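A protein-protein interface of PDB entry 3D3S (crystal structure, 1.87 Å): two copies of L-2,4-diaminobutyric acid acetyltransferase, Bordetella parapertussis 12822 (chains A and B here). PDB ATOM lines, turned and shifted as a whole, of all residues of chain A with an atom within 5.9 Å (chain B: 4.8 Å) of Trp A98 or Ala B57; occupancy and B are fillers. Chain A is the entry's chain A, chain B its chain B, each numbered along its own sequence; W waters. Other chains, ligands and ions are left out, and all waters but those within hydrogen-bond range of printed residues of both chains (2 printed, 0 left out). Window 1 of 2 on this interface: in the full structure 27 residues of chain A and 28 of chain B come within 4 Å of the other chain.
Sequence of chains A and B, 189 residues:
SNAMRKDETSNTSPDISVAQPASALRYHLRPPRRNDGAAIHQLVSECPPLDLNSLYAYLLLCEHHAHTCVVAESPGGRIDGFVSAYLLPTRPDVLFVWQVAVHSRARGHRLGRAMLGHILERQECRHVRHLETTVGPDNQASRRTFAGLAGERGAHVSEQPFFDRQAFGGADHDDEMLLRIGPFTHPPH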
ATOM      1  N   ASN A  53      26.461  16.616  -5.537  1.00  0.00           N
ATOM      2  CA  ASN A  53      25.270  15.809  -5.255  1.00  0.00           C
ATOM      3  C   ASN A  53      24.075  16.458  -5.897  1.00  0.00           C
ATOM      4  O   ASN A  53      24.212  17.535  -6.491  1.00  0.00           O
ATOM      5  CB  ASN A  53      25.114  15.693  -3.732  1.00  0.00           C
ATOM      6  CG  ASN A  53      26.281  14.921  -3.125  1.00  0.00           C
ATOM      7  OD1 ASN A  53      26.361  13.710  -3.271  1.00  0.00           O
ATOM      8  ND2 ASN A  53      27.243  15.634  -2.477  1.00  0.00           N
ATOM      9  N   ALA A  57      19.780  17.144  -2.414  1.00  0.00           N
ATOM     10  CA  ALA A  57      20.678  16.883  -1.275  1.00  0.00           C
ATOM     11  C   ALA A  57      21.077  18.186  -0.621  1.00  0.00           C
ATOM     12  O   ALA A  57      21.089  18.296   0.613  1.00  0.00           O
ATOM     13  CB  ALA A  57      21.986  16.110  -1.714  1.00  0.00           C
ATOM     14  N   TYR A  58      21.363  19.224  -1.422  1.00  0.00           N
ATOM     15  CA  TYR A  58      21.642  20.537  -0.784  1.00  0.00           C
ATOM     16  C   TYR A  58      20.390  21.201  -0.155  1.00  0.00           C
ATOM     17  O   TYR A  58      20.494  21.901   0.906  1.00  0.00           O
ATOM     18  CB  TYR A  58      22.330  21.486  -1.804  1.00  0.00           C
ATOM     19  CG  TYR A  58      23.644  20.850  -2.224  1.00  0.00           C
ATOM     20  CD1 TYR A  58      24.742  20.835  -1.332  1.00  0.00           C
ATOM     21  CD2 TYR A  58      23.752  20.153  -3.436  1.00  0.00           C
ATOM     22  CE1 TYR A  58      25.905  20.182  -1.648  1.00  0.00           C
ATOM     23  CE2 TYR A  58      24.953  19.500  -3.778  1.00  0.00           C
ATOM     24  CZ  TYR A  58      25.981  19.501  -2.892  1.00  0.00           C
ATOM     25  OH  TYR A  58      27.128  18.849  -3.190  1.00  0.00           O
ATOM     26  N   LEU A  61      20.073  19.720   3.275  1.00  0.00           N
ATOM     27  CA  LEU A  61      21.020  20.426   4.190  1.00  0.00           C
ATOM     28  C   LEU A  61      20.461  21.773   4.648  1.00  0.00           C
ATOM     29  O   LEU A  61      20.507  22.125   5.886  1.00  0.00           O
ATOM     30  CB  LEU A  61      22.443  20.593   3.518  1.00  0.00           C
ATOM     31  CG  LEU A  61      23.219  19.247   3.393  1.00  0.00           C
ATOM     32  CD1 LEU A  61      24.404  19.367   2.452  1.00  0.00           C
ATOM     33  CD2 LEU A  61      23.718  18.802   4.829  1.00  0.00           C
ATOM     34  N   VAL A  83      29.950  25.478   3.843  1.00  0.00           N
ATOM     35  CA  VAL A  83      30.376  24.253   4.538  1.00  0.00           C
ATOM     36  C   VAL A  83      29.129  23.456   4.939  1.00  0.00           C
ATOM     37  O   VAL A  83      28.201  24.054   5.537  1.00  0.00           O
ATOM     38  CB  VAL A  83      31.244  24.527   5.785  1.00  0.00           C
ATOM     39  CG1 VAL A  83      31.553  23.104   6.558  1.00  0.00           C
ATOM     40  CG2 VAL A  83      32.568  25.237   5.320  1.00  0.00           C
ATOM     41  N   SER A  84      29.107  22.148   4.615  1.00  0.00           N
ATOM     42  CA  SER A  84      28.067  21.231   5.145  1.00  0.00           C
ATOM     43  C   SER A  84      28.648  20.427   6.257  1.00  0.00           C
ATOM     44  O   SER A  84      29.754  19.890   6.115  1.00  0.00           O
ATOM     45  CB  SER A  84      27.551  20.251   4.088  1.00  0.00           C
ATOM     46  OG  SER A  84      28.644  19.732   3.330  1.00  0.00           O
ATOM     47  N   ALA A  85      27.908  20.346   7.350  1.00  0.00           N
ATOM     48  CA  ALA A  85      28.337  19.587   8.529  1.00  0.00           C
ATOM     49  C   ALA A  85      27.113  19.200   9.341  1.00  0.00           C
ATOM     50  O   ALA A  85      26.043  19.818   9.193  1.00  0.00           O
ATOM     51  CB  ALA A  85      29.314  20.437   9.391  1.00  0.00           C
ATOM     52  N   TYR A  86      27.257  18.170  10.194  1.00  0.00           N
ATOM     53  CA  TYR A  86      26.194  17.775  11.075  1.00  0.00           C
ATOM     54  C   TYR A  86      26.795  17.010  12.229  1.00  0.00           C
ATOM     55  O   TYR A  86      27.891  16.426  12.114  1.00  0.00           O
ATOM     56  CB  TYR A  86      25.186  16.900  10.334  1.00  0.00           C
ATOM     57  CG  TYR A  86      25.765  15.743   9.557  1.00  0.00           C
ATOM     58  CD1 TYR A  86      25.909  14.454  10.150  1.00  0.00           C
ATOM     59  CD2 TYR A  86      26.115  15.888   8.220  1.00  0.00           C
ATOM     60  CE1 TYR A  86      26.438  13.385   9.397  1.00  0.00           C
ATOM     61  CE2 TYR A  86      26.612  14.824   7.449  1.00  0.00           C
ATOM     62  CZ  TYR A  86      26.772  13.579   8.056  1.00  0.00           C
ATOM     63  OH  TYR A  86      27.262  12.539   7.303  1.00  0.00           O
ATOM     64  N   PHE A  96      30.709  16.230  12.113  1.00  0.00           N
ATOM     65  CA  PHE A  96      31.277  15.729  10.875  1.00  0.00           C
ATOM     66  C   PHE A  96      31.137  16.795   9.762  1.00  0.00           C
ATOM     67  O   PHE A  96      30.065  17.286   9.567  1.00  0.00           O
ATOM     68  CB  PHE A  96      30.592  14.437  10.468  1.00  0.00           C
ATOM     69  CG  PHE A  96      31.200  13.854   9.227  1.00  0.00           C
ATOM     70  CD1 PHE A  96      32.342  13.070   9.319  1.00  0.00           C
ATOM     71  CD2 PHE A  96      30.638  14.127   7.968  1.00  0.00           C
ATOM     72  CE1 PHE A  96      32.922  12.528   8.188  1.00  0.00           C
ATOM     73  CE2 PHE A  96      31.230  13.625   6.837  1.00  0.00           C
ATOM     74  CZ  PHE A  96      32.391  12.812   6.972  1.00  0.00           C
ATOM     75  N   VAL A  97      32.239  17.142   9.113  1.00  0.00           N
ATOM     76  CA  VAL A  97      32.284  18.099   8.021  1.00  0.00           C
ATOM     77  C   VAL A  97      32.291  17.317   6.719  1.00  0.00           C
ATOM     78  O   VAL A  97      33.206  16.512   6.449  1.00  0.00           O
ATOM     79  CB  VAL A  97      33.518  18.983   8.127  1.00  0.00           C
ATOM     80  CG1 VAL A  97      33.626  19.929   6.830  1.00  0.00           C
ATOM     81  CG2 VAL A  97      33.415  19.776   9.380  1.00  0.00           C
ATOM     82  N   TRP A  98      31.264  17.560   5.905  1.00  0.00           N
ATOM     83  CA  TRP A  98      31.055  16.765   4.669  1.00  0.00           C
ATOM     84  C   TRP A  98      31.743  17.470   3.529  1.00  0.00           C
ATOM     85  O   TRP A  98      32.641  16.876   2.943  1.00  0.00           O
ATOM     86  CB  TRP A  98      29.551  16.582   4.413  1.00  0.00           C
ATOM     87  CG  TRP A  98      29.144  15.929   3.154  1.00  0.00           C
ATOM     88  CD1 TRP A  98      29.946  15.381   2.152  1.00  0.00           C
ATOM     89  CD2 TRP A  98      27.811  15.678   2.782  1.00  0.00           C
ATOM     90  NE1 TRP A  98      29.138  14.835   1.172  1.00  0.00           N
ATOM     91  CE2 TRP A  98      27.826  15.027   1.539  1.00  0.00           C
ATOM     92  CE3 TRP A  98      26.590  16.030   3.356  1.00  0.00           C
ATOM     93  CZ2 TRP A  98      26.657  14.677   0.876  1.00  0.00           C
ATOM     94  CZ3 TRP A  98      25.401  15.652   2.740  1.00  0.00           C
ATOM     95  CH2 TRP A  98      25.440  15.000   1.486  1.00  0.00           C
ATOM     96  N   GLN A  99      31.338  18.707   3.177  1.00  0.00           N
ATOM     97  CA  GLN A  99      32.000  19.435   2.069  1.00  0.00           C
ATOM     98  C   GLN A  99      32.393  20.850   2.492  1.00  0.00           C
ATOM     99  O   GLN A  99      31.639  21.510   3.231  1.00  0.00           O
ATOM    100  CB  GLN A  99      31.043  19.523   0.856  1.00  0.00           C
ATOM    101  CG  GLN A  99      30.783  18.136   0.275  1.00  0.00           C
ATOM    102  CD  GLN A  99      30.097  18.237  -1.062  1.00  0.00           C
ATOM    103  OE1 GLN A  99      28.990  18.759  -1.152  1.00  0.00           O
ATOM    104  NE2 GLN A  99      30.738  17.693  -2.110  1.00  0.00           N
ATOM    105  N   VAL A 100      33.571  21.296   2.036  1.00  0.00           N
ATOM    106  CA  VAL A 100      34.014  22.688   2.196  1.00  0.00           C
ATOM    107  C   VAL A 100      34.219  23.221   0.802  1.00  0.00           C
ATOM    108  O   VAL A 100      35.133  22.785   0.078  1.00  0.00           O
ATOM    109  CB  VAL A 100      35.322  22.766   2.986  1.00  0.00           C
ATOM    110  CG1 VAL A 100      35.793  24.261   3.191  1.00  0.00           C
ATOM    111  CG2 VAL A 100      35.128  22.054   4.315  1.00  0.00           C
ATOM    112  N   GLU A 132      35.325  15.541  12.743  1.00  0.00           N
ATOM    113  CA  GLU A 132      35.745  14.497  11.804  1.00  0.00           C
ATOM    114  C   GLU A 132      35.481  14.962  10.372  1.00  0.00           C
ATOM    115  O   GLU A 132      34.520  15.674  10.128  1.00  0.00           O
ATOM    116  CB  GLU A 132      34.915  13.223  12.062  1.00  0.00           C
ATOM    117  CG  GLU A 132      35.539  12.378  13.115  1.00  0.00           C
ATOM    118  CD  GLU A 132      34.836  11.062  13.452  1.00  0.00           C
ATOM    119  OE1 GLU A 132      34.007  10.509  12.684  1.00  0.00           O
ATOM    120  OE2 GLU A 132      35.162  10.562  14.538  1.00  0.00           O
ATOM    121  N   THR A 133      36.307  14.553   9.424  1.00  0.00           N
ATOM    122  CA  THR A 133      36.068  14.907   8.061  1.00  0.00           C
ATOM    123  C   THR A 133      36.922  13.925   7.263  1.00  0.00           C
ATOM    124  O   THR A 133      37.705  13.178   7.856  1.00  0.00           O
ATOM    125  CB  THR A 133      36.486  16.361   7.777  1.00  0.00           C
ATOM    126  OG1 THR A 133      35.925  16.771   6.513  1.00  0.00           O
ATOM    127  CG2 THR A 133      38.043  16.494   7.691  1.00  0.00           C
ATOM    128  N   THR A 134      36.819  13.929   5.949  1.00  0.00           N
ATOM    129  CA  THR A 134      37.765  13.108   5.189  1.00  0.00           C
ATOM    130  C   THR A 134      38.541  13.943   4.175  1.00  0.00           C
ATOM    131  O   THR A 134      38.088  15.069   3.757  1.00  0.00           O
ATOM    132  CB  THR A 134      37.116  11.926   4.464  1.00  0.00           C
ATOM    133  OG1 THR A 134      36.351  12.440   3.367  1.00  0.00           O
ATOM    134  CG2 THR A 134      36.211  11.079   5.411  1.00  0.00           C
ATOM    135  N   ASN B  53      22.786  10.545  -6.231  1.00  0.00           N
ATOM    136  CA  ASN B  53      23.797  11.336  -5.461  1.00  0.00           C
ATOM    137  C   ASN B  53      25.189  10.729  -5.604  1.00  0.00           C
ATOM    138  O   ASN B  53      25.300   9.673  -6.208  1.00  0.00           O
ATOM    139  CB  ASN B  53      23.345  11.395  -4.038  1.00  0.00           C
ATOM    140  CG  ASN B  53      22.110  12.260  -3.907  1.00  0.00           C
ATOM    141  OD1 ASN B  53      22.178  13.464  -4.092  1.00  0.00           O
ATOM    142  ND2 ASN B  53      20.984  11.646  -3.653  1.00  0.00           N
ATOM    143  N   SER B  54      26.239  11.399  -5.123  1.00  0.00           N
ATOM    144  CA  SER B  54      27.618  10.886  -5.295  1.00  0.00           C
ATOM    145  C   SER B  54      27.730   9.585  -4.497  1.00  0.00           C
ATOM    146  O   SER B  54      27.036   9.401  -3.472  1.00  0.00           O
ATOM    147  CB  SER B  54      28.630  11.921  -4.743  1.00  0.00           C
ATOM    148  OG  SER B  54      28.401  12.043  -3.293  1.00  0.00           O
ATOM    149  N   LEU B  55      28.578   8.660  -4.957  1.00  0.00           N
ATOM    150  CA  LEU B  55      28.885   7.484  -4.160  1.00  0.00           C
ATOM    151  C   LEU B  55      29.249   7.795  -2.706  1.00  0.00           C
ATOM    152  O   LEU B  55      28.765   7.100  -1.826  1.00  0.00           O
ATOM    153  CB  LEU B  55      29.989   6.695  -4.849  1.00  0.00           C
ATOM    154  CG  LEU B  55      30.472   5.314  -4.293  1.00  0.00           C
ATOM    155  CD1 LEU B  55      29.530   4.612  -3.437  1.00  0.00           C
ATOM    156  CD2 LEU B  55      30.875   4.452  -5.507  1.00  0.00           C
ATOM    157  N   TYR B  56      30.054   8.842  -2.483  1.00  0.00           N
ATOM    158  CA  TYR B  56      30.449   9.266  -1.145  1.00  0.00           C
ATOM    159  C   TYR B  56      29.221   9.559  -0.307  1.00  0.00           C
ATOM    160  O   TYR B  56      29.208   9.234   0.868  1.00  0.00           O
ATOM    161  CB  TYR B  56      31.304  10.507  -1.266  1.00  0.00           C
ATOM    162  CG  TYR B  56      31.971  10.950  -0.006  1.00  0.00           C
ATOM    163  CD1 TYR B  56      31.338  11.889   0.822  1.00  0.00           C
ATOM    164  CD2 TYR B  56      33.267  10.502   0.343  1.00  0.00           C
ATOM    165  CE1 TYR B  56      31.923  12.362   1.971  1.00  0.00           C
ATOM    166  CE2 TYR B  56      33.896  11.006   1.518  1.00  0.00           C
ATOM    167  CZ  TYR B  56      33.184  11.932   2.337  1.00  0.00           C
ATOM    168  OH  TYR B  56      33.742  12.458   3.509  1.00  0.00           O
ATOM    169  N   ALA B  57      28.202  10.228  -0.876  1.00  0.00           N
ATOM    170  CA  ALA B  57      26.995  10.427  -0.077  1.00  0.00           C
ATOM    171  C   ALA B  57      26.335   9.169   0.437  1.00  0.00           C
ATOM    172  O   ALA B  57      25.873   9.154   1.604  1.00  0.00           O
ATOM    173  CB  ALA B  57      25.924  11.331  -0.846  1.00  0.00           C
ATOM    174  N   TYR B  58      26.234   8.129  -0.415  1.00  0.00           N
ATOM    175  CA  TYR B  58      25.739   6.837   0.033  1.00  0.00           C
ATOM    176  C   TYR B  58      26.630   6.205   1.113  1.00  0.00           C
ATOM    177  O   TYR B  58      26.122   5.617   2.084  1.00  0.00           O
ATOM    178  CB  TYR B  58      25.448   5.888  -1.150  1.00  0.00           C
ATOM    179  CG  TYR B  58      24.328   6.489  -2.017  1.00  0.00           C
ATOM    180  CD1 TYR B  58      22.996   6.512  -1.555  1.00  0.00           C
ATOM    181  CD2 TYR B  58      24.643   7.088  -3.206  1.00  0.00           C
ATOM    182  CE1 TYR B  58      21.944   7.142  -2.303  1.00  0.00           C
ATOM    183  CE2 TYR B  58      23.652   7.759  -3.940  1.00  0.00           C
ATOM    184  CZ  TYR B  58      22.301   7.762  -3.476  1.00  0.00           C
ATOM    185  OH  TYR B  58      21.389   8.463  -4.232  1.00  0.00           O
ATOM    186  N   LEU B  59      27.940   6.329   0.957  1.00  0.00           N
ATOM    187  CA  LEU B  59      28.841   5.838   2.016  1.00  0.00           C
ATOM    188  C   LEU B  59      28.607   6.541   3.364  1.00  0.00           C
ATOM    189  O   LEU B  59      28.625   5.907   4.417  1.00  0.00           O
ATOM    190  CB  LEU B  59      30.291   5.995   1.565  1.00  0.00           C
ATOM    191  CG  LEU B  59      30.691   4.955   0.490  1.00  0.00           C
ATOM    192  CD1 LEU B  59      32.097   5.469   0.079  1.00  0.00           C
ATOM    193  CD2 LEU B  59      30.801   3.535   1.079  1.00  0.00           C
ATOM    194  N   LEU B  60      28.332   7.831   3.343  1.00  0.00           N
ATOM    195  CA  LEU B  60      28.020   8.570   4.575  1.00  0.00           C
ATOM    196  C   LEU B  60      26.736   8.083   5.201  1.00  0.00           C
ATOM    197  O   LEU B  60      26.647   7.984   6.426  1.00  0.00           O
ATOM    198  CB  LEU B  60      27.849  10.072   4.281  1.00  0.00           C
ATOM    199  CG  LEU B  60      29.155  10.856   3.975  1.00  0.00           C
ATOM    200  CD1 LEU B  60      28.817  12.355   3.898  1.00  0.00           C
ATOM    201  CD2 LEU B  60      30.354  10.644   4.909  1.00  0.00           C
ATOM    202  N   LEU B  61      25.734   7.754   4.381  1.00  0.00           N
ATOM    203  CA  LEU B  61      24.526   7.123   4.938  1.00  0.00           C
ATOM    204  C   LEU B  61      24.901   5.812   5.653  1.00  0.00           C
ATOM    205  O   LEU B  61      24.411   5.540   6.764  1.00  0.00           O
ATOM    206  CB  LEU B  61      23.438   6.858   3.917  1.00  0.00           C
ATOM    207  CG  LEU B  61      22.837   8.204   3.397  1.00  0.00           C
ATOM    208  CD1 LEU B  61      22.179   7.969   2.012  1.00  0.00           C
ATOM    209  CD2 LEU B  61      21.837   8.733   4.464  1.00  0.00           C
HETATM  210  O   HOH W   1      34.339  14.908   4.494  1.00  0.00           O
HETATM  211  O   HOH W   2      29.691  14.099  -1.622  1.00  0.00           O
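Asn B53 touches its own counterpart, Asn A53.
Asn A53 touches Ala B57, and with the chains exchanged Ala A57 touches Asn B53.
Positions printed for both chains: 53, 57, 58 and 61.
Hydrophobic or aromatic side chains of chain B within 4 Å of the printed part of chain A: Tyr B56, Ala B57 and Leu B60.
Hydrophobic or aromatic side chains of chain A that line the printed part of chain B: Ala A57, Tyr A86, Phe A96 and Trp A98.
Among the printed residues, 11 pairs touch across the chains.
Among the printed residues, no Asp or Glu carboxylate lies within 4 Å of a Lys or Arg side-chain nitrogen of the other chain.
The backbone carbonyl oxygen of Ser A84 sits at hydrogen-bond distance from the backbone NH of Trp A98, at 2.8 Å.
The side-chain hydroxyl (OH) of Tyr A58 sits at hydrogen-bond distance from the side-chain amide nitrogen (ND2) of Asn A53 (3.3 Å).
The backbone carbonyl oxygen (O) of Tyr A86 lies within hydrogen-bond range of the backbone NH (N) of Phe A96 (2.8 Å).
The backbone NH of Ala B57 is in hydrogen-bond range of the side-chain hydroxyl of Ser B54 (3.0 Å).
The backbone NH (N) of Asn B53 sits at hydrogen-bond distance from the side-chain hydroxyl (OH) of Tyr B58, 3.2 Å away.
Trp A98 touches three residues of chain B.
Printed residues of chain A within 4 Å of Leu B60: Tyr A86, Phe A96 and Trp A98.
Printed residues of chain B within 4 Å of Thr A134: Tyr B56 (2.6 Å).
Printed residues of chain B within 4 Å of Ala A57: Asn B53.
Of the printed residues of chain A, Tyr B56 touches Phe A96, Trp A98 and Thr A134.
Of the printed residues of chain A, Asn B53 touches Asn A53 (3.7 Å) and Ala A57 (3.6 Å).
The nearest printed residue of chain B that does not touch Trp A98 is Ser B54 (5.2 Å).
The nearest printed residue of chain B that does not touch Phe A96 is Leu B59 (8.2 Å).
The side-chain hydroxyl of Thr A134 is in hydrogen-bond range of the side-chain hydroxyl of Tyr B56.
OD1 of Asn A53 is in hydrogen-bond range of OG of Ser B54.
OD1 of Asn B53 touches CB of Asn A53 (3.7 Å).
Ala B57 touches Asn A53 (CB to OD1, 3.4 Å).
Asn B53 touches Ala A57 (OD1 to CB, 3.6 Å).
Tyr A86 touches Leu B60 (OH to CD1, 3.7 Å).
Phe A96 touches Tyr B56.
Phe A96 touches Leu B60 (CZ to CD2, 3.6 Å).
Tyr B56 touches Trp A98 (CE1 to CD1, 3.6 Å).
CB of Ala B57 touches CZ2 of Trp A98, at 3.8 Å.
Leu B60 touches Trp A98.
Water W1 lies within hydrogen-bond range of OH of Tyr B56 (2.7 Å), O of Val A97 (2.8 Å), O of Trp A98 (3.0 Å), N of Thr A134 (3.0 Å) and OG1 of Thr A133 (3.2 Å).
Water W2 lies within hydrogen-bond range of the indole nitrogen of Trp A98 (2.9 Å), the side-chain hydroxyl of Ser B54 (2.9 Å) and the side-chain amide nitrogen of Asn A53 (3.0 Å).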
